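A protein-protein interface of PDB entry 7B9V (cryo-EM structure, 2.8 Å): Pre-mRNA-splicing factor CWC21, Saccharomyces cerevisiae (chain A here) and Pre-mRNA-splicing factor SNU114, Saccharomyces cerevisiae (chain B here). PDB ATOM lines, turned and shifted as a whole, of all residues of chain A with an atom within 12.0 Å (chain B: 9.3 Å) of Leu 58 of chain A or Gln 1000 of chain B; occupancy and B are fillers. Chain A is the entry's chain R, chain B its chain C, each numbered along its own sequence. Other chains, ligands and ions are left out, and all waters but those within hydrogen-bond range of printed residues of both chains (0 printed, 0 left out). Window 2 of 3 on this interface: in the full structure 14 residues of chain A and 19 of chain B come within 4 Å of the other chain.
Of the 12 printed residues of chain A, 4 touch a printed residue of chain B.
Printed residues of chain A that touch a printed residue of chain B: Leu 58, Val 60, Gln 63 and Ile 64.
Among the printed residues, 8 pairs touch across the chains.
Leu 58 of chain A touches Gln 1000 of chain B.
CD2 of Leu 58 of chain A touches N of Leu 1001 of chain B, at 3.9 Å.
Val 60 of chain A touches Ala 687 of chain B (O to CB, 3.8 Å).
Val 60 of chain A touches Ile 689 of chain B.
Ile 64 of chain A touches Phe 686 of chain B (CD1 to O, 3.7 Å).
Ile 64 of chain A touches Ala 687 of chain B (CD1 to CA, 3.7 Å).
Ile 64 of chain A touches Ser 688 of chain B.
The side-chain amide oxygen of Gln 63 of chain A lies close to the backbone carbonyl oxygen of Ser 688 of chain B (3.4 Å).
No residue of chain B comes within 4 Å of Pro 57 of chain A.
Leu 58 of chain A touches just these residues of chain B: Gln 1000 and Leu 1001.
Ala 59 of chain A touches none of the printed residues of chain B.
Printed residues of chain A within 4 Å of Phe 686 of chain B: Ile 64 (3.7 Å).
Of the printed residues of chain A, Ala 687 of chain B touches Val 60 (3.8 Å) and Ile 64 (3.7 Å).
No residue of chain A comes within 4 Å of Leu 997 of chain B.
Of chain A, only Leu 58 comes within 4 Å of Gln 1000 of chain B.
No residue of chain A comes within 4 Å of Arg 1002 of chain B.
No residue of chain A comes within 4 Å of Asn 1004 of chain B.
Gly 1005 of chain B touches none of the printed residues of chain A.
The nearest printed residue of chain B that does not touch Gln 63 of chain A is Ile 689 of chain B (4.5 Å).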
ATOM      1  N   ARG A  56      31.173  23.888   6.333  1.00  0.00           N
ATOM      2  CA  ARG A  56      30.085  24.865   6.411  1.00  0.00           C
ATOM      3  C   ARG A  56      28.703  24.239   5.957  1.00  0.00           C
ATOM      4  O   ARG A  56      27.734  24.419   6.691  1.00  0.00           O
ATOM      5  CB  ARG A  56      30.477  26.152   5.620  1.00  0.00           C
ATOM      6  CG  ARG A  56      29.391  27.199   5.444  1.00  0.00           C
ATOM      7  CD  ARG A  56      28.853  27.713   6.759  1.00  0.00           C
ATOM      8  NE  ARG A  56      29.892  28.533   7.369  1.00  0.00           N
ATOM      9  CZ  ARG A  56      29.905  28.944   8.628  1.00  0.00           C
ATOM     10  NH1 ARG A  56      28.942  28.616   9.469  1.00  0.00           N
ATOM     11  NH2 ARG A  56      30.903  29.719   9.047  1.00  0.00           N
ATOM     12  N   PRO A  57      28.558  23.533   4.818  1.00  0.00           N
ATOM     13  CA  PRO A  57      27.308  22.790   4.601  1.00  0.00           C
ATOM     14  C   PRO A  57      27.282  21.477   5.369  1.00  0.00           C
ATOM     15  O   PRO A  57      28.314  20.912   5.733  1.00  0.00           O
ATOM     16  CB  PRO A  57      27.282  22.515   3.104  1.00  0.00           C
ATOM     17  CG  PRO A  57      28.659  22.474   2.735  1.00  0.00           C
ATOM     18  CD  PRO A  57      29.370  23.451   3.569  1.00  0.00           C
ATOM     19  N   LEU A  58      26.070  21.001   5.624  1.00  0.00           N
ATOM     20  CA  LEU A  58      25.891  19.687   6.224  1.00  0.00           C
ATOM     21  C   LEU A  58      26.076  18.631   5.131  1.00  0.00           C
ATOM     22  O   LEU A  58      26.053  18.947   3.939  1.00  0.00           O
ATOM     23  CB  LEU A  58      24.503  19.585   6.882  1.00  0.00           C
ATOM     24  CG  LEU A  58      24.093  18.391   7.763  1.00  0.00           C
ATOM     25  CD1 LEU A  58      25.087  18.204   8.907  1.00  0.00           C
ATOM     26  CD2 LEU A  58      22.673  18.530   8.279  1.00  0.00           C
ATOM     27  N   ALA A  59      26.370  17.393   5.561  1.00  0.00           N
ATOM     28  CA  ALA A  59      26.714  16.302   4.649  1.00  0.00           C
ATOM     29  C   ALA A  59      25.581  15.996   3.678  1.00  0.00           C
ATOM     30  O   ALA A  59      25.837  15.724   2.499  1.00  0.00           O
ATOM     31  CB  ALA A  59      27.083  15.052   5.449  1.00  0.00           C
ATOM     32  N   VAL A  60      24.336  15.978   4.166  1.00  0.00           N
ATOM     33  CA  VAL A  60      23.205  15.674   3.294  1.00  0.00           C
ATOM     34  C   VAL A  60      22.977  16.763   2.247  1.00  0.00           C
ATOM     35  O   VAL A  60      22.364  16.484   1.210  1.00  0.00           O
ATOM     36  CB  VAL A  60      21.909  15.432   4.096  1.00  0.00           C
ATOM     37  CG1 VAL A  60      21.972  14.100   4.835  1.00  0.00           C
ATOM     38  CG2 VAL A  60      21.641  16.574   5.063  1.00  0.00           C
ATOM     39  N   GLN A  61      23.413  18.008   2.510  1.00  0.00           N
ATOM     40  CA  GLN A  61      23.294  19.071   1.513  1.00  0.00           C
ATOM     41  C   GLN A  61      24.173  18.793   0.296  1.00  0.00           C
ATOM     42  O   GLN A  61      23.777  19.087  -0.842  1.00  0.00           O
ATOM     43  CB  GLN A  61      23.641  20.424   2.143  1.00  0.00           C
ATOM     44  CG  GLN A  61      23.606  21.609   1.176  1.00  0.00           C
ATOM     45  CD  GLN A  61      23.645  22.958   1.857  1.00  0.00           C
ATOM     46  OE1 GLN A  61      23.564  23.059   3.081  1.00  0.00           O
ATOM     47  NE2 GLN A  61      23.773  24.012   1.059  1.00  0.00           N
ATOM     48  N   LYS A  62      25.355  18.185   0.511  1.00  0.00           N
ATOM     49  CA  LYS A  62      26.280  17.898  -0.588  1.00  0.00           C
ATOM     50  C   LYS A  62      25.734  16.846  -1.560  1.00  0.00           C
ATOM     51  O   LYS A  62      26.225  16.749  -2.691  1.00  0.00           O
ATOM     52  CB  LYS A  62      27.635  17.453  -0.003  1.00  0.00           C
ATOM     53  CG  LYS A  62      28.827  17.451  -0.969  1.00  0.00           C
ATOM     54  CD  LYS A  62      30.157  17.175  -0.311  1.00  0.00           C
ATOM     55  CE  LYS A  62      31.258  17.283  -1.343  1.00  0.00           C
ATOM     56  NZ  LYS A  62      32.578  17.077  -0.716  1.00  0.00           N
ATOM     57  N   GLN A  63      24.691  16.099  -1.170  1.00  0.00           N
ATOM     58  CA  GLN A  63      24.186  15.036  -2.029  1.00  0.00           C
ATOM     59  C   GLN A  63      23.471  15.584  -3.260  1.00  0.00           C
ATOM     60  O   GLN A  63      23.434  14.904  -4.291  1.00  0.00           O
ATOM     61  CB  GLN A  63      23.282  14.109  -1.221  1.00  0.00           C
ATOM     62  CG  GLN A  63      24.045  13.388  -0.118  1.00  0.00           C
ATOM     63  CD  GLN A  63      23.227  12.320   0.566  1.00  0.00           C
ATOM     64  OE1 GLN A  63      21.999  12.359   0.550  1.00  0.00           O
ATOM     65  NE2 GLN A  63      23.906  11.349   1.169  1.00  0.00           N
ATOM     66  N   ILE A  64      22.846  16.770  -3.154  1.00  0.00           N
ATOM     67  CA  ILE A  64      22.322  17.445  -4.344  1.00  0.00           C
ATOM     68  C   ILE A  64      23.468  17.780  -5.297  1.00  0.00           C
ATOM     69  O   ILE A  64      23.368  17.579  -6.524  1.00  0.00           O
ATOM     70  CB  ILE A  64      21.512  18.692  -3.927  1.00  0.00           C
ATOM     71  CG1 ILE A  64      20.227  18.274  -3.208  1.00  0.00           C
ATOM     72  CG2 ILE A  64      21.181  19.600  -5.103  1.00  0.00           C
ATOM     73  CD1 ILE A  64      19.554  19.402  -2.487  1.00  0.00           C
ATOM     74  N   GLU A  65      24.576  18.304  -4.733  1.00  0.00           N
ATOM     75  CA  GLU A  65      25.764  18.648  -5.511  1.00  0.00           C
ATOM     76  C   GLU A  65      26.376  17.418  -6.166  1.00  0.00           C
ATOM     77  O   GLU A  65      26.940  17.511  -7.261  1.00  0.00           O
ATOM     78  CB  GLU A  65      26.801  19.350  -4.627  1.00  0.00           C
ATOM     79  CG  GLU A  65      26.322  20.606  -3.884  1.00  0.00           C
ATOM     80  CD  GLU A  65      26.188  21.875  -4.743  1.00  0.00           C
ATOM     81  OE1 GLU A  65      26.242  21.831  -5.995  1.00  0.00           O
ATOM     82  OE2 GLU A  65      26.019  22.954  -4.137  1.00  0.00           O
ATOM     83  N   THR A  66      26.268  16.261  -5.501  1.00  0.00           N
ATOM     84  CA  THR A  66      26.689  15.007  -6.110  1.00  0.00           C
ATOM     85  C   THR A  66      25.749  14.616  -7.239  1.00  0.00           C
ATOM     86  O   THR A  66      26.201  14.155  -8.298  1.00  0.00           O
ATOM     87  CB  THR A  66      26.735  13.912  -5.038  1.00  0.00           C
ATOM     88  OG1 THR A  66      27.593  14.325  -3.968  1.00  0.00           O
ATOM     89  CG2 THR A  66      27.251  12.588  -5.599  1.00  0.00           C
ATOM     90  N   HIS A  67      24.434  14.793  -7.015  1.00  0.00           N
ATOM     91  CA  HIS A  67      23.430  14.359  -7.983  1.00  0.00           C
ATOM     92  C   HIS A  67      23.517  15.124  -9.297  1.00  0.00           C
ATOM     93  O   HIS A  67      23.179  14.561 -10.345  1.00  0.00           O
ATOM     94  CB  HIS A  67      22.031  14.484  -7.360  1.00  0.00           C
ATOM     95  CG  HIS A  67      20.905  14.168  -8.302  1.00  0.00           C
ATOM     96  ND1 HIS A  67      20.637  12.889  -8.735  1.00  0.00           N
ATOM     97  CD2 HIS A  67      19.930  14.953  -8.823  1.00  0.00           C
ATOM     98  CE1 HIS A  67      19.579  12.904  -9.524  1.00  0.00           C
ATOM     99  NE2 HIS A  67      19.126  14.142  -9.588  1.00  0.00           N
ATOM    100  N   PHE B 686      16.091  21.867   0.400  1.00  0.00           N
ATOM    101  CA  PHE B 686      17.457  22.275   0.734  1.00  0.00           C
ATOM    102  C   PHE B 686      18.411  21.092   0.864  1.00  0.00           C
ATOM    103  O   PHE B 686      19.629  21.282   0.748  1.00  0.00           O
ATOM    104  CB  PHE B 686      17.481  23.151   2.014  1.00  0.00           C
ATOM    105  CG  PHE B 686      16.980  22.469   3.293  1.00  0.00           C
ATOM    106  CD1 PHE B 686      17.791  21.627   4.058  1.00  0.00           C
ATOM    107  CD2 PHE B 686      15.711  22.750   3.763  1.00  0.00           C
ATOM    108  CE1 PHE B 686      17.313  21.024   5.207  1.00  0.00           C
ATOM    109  CE2 PHE B 686      15.224  22.160   4.917  1.00  0.00           C
ATOM    110  CZ  PHE B 686      16.028  21.298   5.641  1.00  0.00           C
ATOM    111  N   ALA B 687      17.886  19.888   1.087  1.00  0.00           N
ATOM    112  CA  ALA B 687      18.699  18.685   1.087  1.00  0.00           C
ATOM    113  C   ALA B 687      17.831  17.493   0.723  1.00  0.00           C
ATOM    114  O   ALA B 687      16.699  17.360   1.196  1.00  0.00           O
ATOM    115  CB  ALA B 687      19.352  18.458   2.454  1.00  0.00           C
ATOM    116  N   SER B 688      18.380  16.639  -0.137  1.00  0.00           N
ATOM    117  CA  SER B 688      17.717  15.418  -0.591  1.00  0.00           C
ATOM    118  C   SER B 688      18.100  14.250   0.317  1.00  0.00           C
ATOM    119  O   SER B 688      18.828  13.339  -0.082  1.00  0.00           O
ATOM    120  CB  SER B 688      18.076  15.135  -2.044  1.00  0.00           C
ATOM    121  OG  SER B 688      17.328  14.047  -2.554  1.00  0.00           O
ATOM    122  N   ILE B 689      17.649  14.322   1.571  1.00  0.00           N
ATOM    123  CA  ILE B 689      18.120  13.399   2.608  1.00  0.00           C
ATOM    124  C   ILE B 689      17.536  12.013   2.331  1.00  0.00           C
ATOM    125  O   ILE B 689      16.487  11.907   1.679  1.00  0.00           O
ATOM    126  CB  ILE B 689      17.796  13.912   4.027  1.00  0.00           C
ATOM    127  CG1 ILE B 689      16.352  13.662   4.434  1.00  0.00           C
ATOM    128  CG2 ILE B 689      18.081  15.394   4.135  1.00  0.00           C
ATOM    129  CD1 ILE B 689      16.112  14.018   5.869  1.00  0.00           C
ATOM    130  N   ILE B 993      12.386  12.608  10.717  1.00  0.00           N
ATOM    131  CA  ILE B 993      13.798  12.370  10.440  1.00  0.00           C
ATOM    132  C   ILE B 993      14.520  12.132  11.760  1.00  0.00           C
ATOM    133  O   ILE B 993      13.986  12.414  12.838  1.00  0.00           O
ATOM    134  CB  ILE B 993      14.439  13.516   9.614  1.00  0.00           C
ATOM    135  CG1 ILE B 993      14.819  14.728  10.460  1.00  0.00           C
ATOM    136  CG2 ILE B 993      13.497  13.986   8.510  1.00  0.00           C
ATOM    137  CD1 ILE B 993      15.634  15.758   9.673  1.00  0.00           C
ATOM    138  N   SER B 994      15.718  11.537  11.664  1.00  0.00           N
ATOM    139  CA  SER B 994      16.506  11.171  12.840  1.00  0.00           C
ATOM    140  C   SER B 994      16.906  12.406  13.640  1.00  0.00           C
ATOM    141  O   SER B 994      17.028  13.506  13.090  1.00  0.00           O
ATOM    142  CB  SER B 994      17.761  10.401  12.424  1.00  0.00           C
ATOM    143  N   ALA B 995      17.059  12.215  14.960  1.00  0.00           N
ATOM    144  CA  ALA B 995      17.288  13.334  15.873  1.00  0.00           C
ATOM    145  C   ALA B 995      18.613  14.033  15.607  1.00  0.00           C
ATOM    146  O   ALA B 995      18.701  15.264  15.741  1.00  0.00           O
ATOM    147  CB  ALA B 995      17.232  12.839  17.317  1.00  0.00           C
ATOM    148  N   GLU B 996      19.670  13.257  15.316  1.00  0.00           N
ATOM    149  CA  GLU B 996      20.966  13.849  14.992  1.00  0.00           C
ATOM    150  C   GLU B 996      20.877  14.698  13.732  1.00  0.00           C
ATOM    151  O   GLU B 996      21.431  15.805  13.682  1.00  0.00           O
ATOM    152  CB  GLU B 996      22.016  12.752  14.827  1.00  0.00           C
ATOM    153  N   LEU B 997      20.181  14.180  12.704  1.00  0.00           N
ATOM    154  CA  LEU B 997      19.977  14.926  11.467  1.00  0.00           C
ATOM    155  C   LEU B 997      19.167  16.190  11.709  1.00  0.00           C
ATOM    156  O   LEU B 997      19.456  17.238  11.121  1.00  0.00           O
ATOM    157  CB  LEU B 997      19.284  14.042  10.430  1.00  0.00           C
ATOM    158  N   TYR B 998      18.115  16.087  12.539  1.00  0.00           N
ATOM    159  CA  TYR B 998      17.250  17.232  12.811  1.00  0.00           C
ATOM    160  C   TYR B 998      18.001  18.337  13.542  1.00  0.00           C
ATOM    161  O   TYR B 998      17.869  19.520  13.198  1.00  0.00           O
ATOM    162  CB  TYR B 998      16.024  16.805  13.620  1.00  0.00           C
ATOM    163  CG  TYR B 998      15.106  17.967  13.950  1.00  0.00           C
ATOM    164  CD1 TYR B 998      14.405  18.628  12.944  1.00  0.00           C
ATOM    165  CD2 TYR B 998      14.956  18.416  15.262  1.00  0.00           C
ATOM    166  CE1 TYR B 998      13.574  19.698  13.233  1.00  0.00           C
ATOM    167  CE2 TYR B 998      14.124  19.488  15.561  1.00  0.00           C
ATOM    168  CZ  TYR B 998      13.437  20.122  14.542  1.00  0.00           C
ATOM    169  OH  TYR B 998      12.611  21.184  14.831  1.00  0.00           O
ATOM    170  N   ALA B 999      18.755  17.966  14.591  1.00  0.00           N
ATOM    171  CA  ALA B 999      19.532  18.952  15.336  1.00  0.00           C
ATOM    172  C   ALA B 999      20.631  19.566  14.481  1.00  0.00           C
ATOM    173  O   ALA B 999      20.921  20.765  14.608  1.00  0.00           O
ATOM    174  CB  ALA B 999      20.124  18.312  16.590  1.00  0.00           C
ATOM    175  N   GLN B1000      21.276  18.749  13.629  1.00  0.00           N
ATOM    176  CA  GLN B1000      22.304  19.267  12.731  1.00  0.00           C
ATOM    177  C   GLN B1000      21.718  20.243  11.722  1.00  0.00           C
ATOM    178  O   GLN B1000      22.352  21.249  11.383  1.00  0.00           O
ATOM    179  CB  GLN B1000      23.004  18.111  12.021  1.00  0.00           C
ATOM    180  N   LEU B1001      20.520  19.933  11.202  1.00  0.00           N
ATOM    181  CA  LEU B1001      19.844  20.833  10.275  1.00  0.00           C
ATOM    182  C   LEU B1001      19.436  22.128  10.958  1.00  0.00           C
ATOM    183  O   LEU B1001      19.479  23.199  10.340  1.00  0.00           O
ATOM    184  CB  LEU B1001      18.626  20.137   9.669  1.00  0.00           C
ATOM    185  N   ARG B1002      18.974  22.031  12.216  1.00  0.00           N
ATOM    186  CA  ARG B1002      18.595  23.221  12.974  1.00  0.00           C
ATOM    187  C   ARG B1002      19.795  24.118  13.235  1.00  0.00           C
ATOM    188  O   ARG B1002      19.681  25.350  13.194  1.00  0.00           O
ATOM    189  CB  ARG B1002      17.932  22.813  14.289  1.00  0.00           C
ATOM    190  N   GLU B1003      20.952  23.512  13.533  1.00  0.00           N
ATOM    191  CA  GLU B1003      22.170  24.288  13.748  1.00  0.00           C
ATOM    192  C   GLU B1003      22.658  24.921  12.450  1.00  0.00           C
ATOM    193  O   GLU B1003      22.970  26.116  12.406  1.00  0.00           O
ATOM    194  CB  GLU B1003      23.254  23.399  14.358  1.00  0.00           C
ATOM    195  N   ASN B1004      22.721  24.124  11.376  1.00  0.00           N
ATOM    196  CA  ASN B1004      23.215  24.595  10.088  1.00  0.00           C
ATOM    197  C   ASN B1004      22.240  25.528   9.383  1.00  0.00           C
ATOM    198  O   ASN B1004      22.674  26.360   8.580  1.00  0.00           O
ATOM    199  CB  ASN B1004      23.538  23.404   9.183  1.00  0.00           C
ATOM    200  N   GLY B1005      20.947  25.431   9.686  1.00  0.00           N
ATOM    201  CA  GLY B1005      19.939  26.269   9.062  1.00  0.00           C
ATOM    202  C   GLY B1005      19.725  25.931   7.596  1.00  0.00           C
ATOM    203  O   GLY B1005      19.108  26.691   6.851  1.00  0.00           O
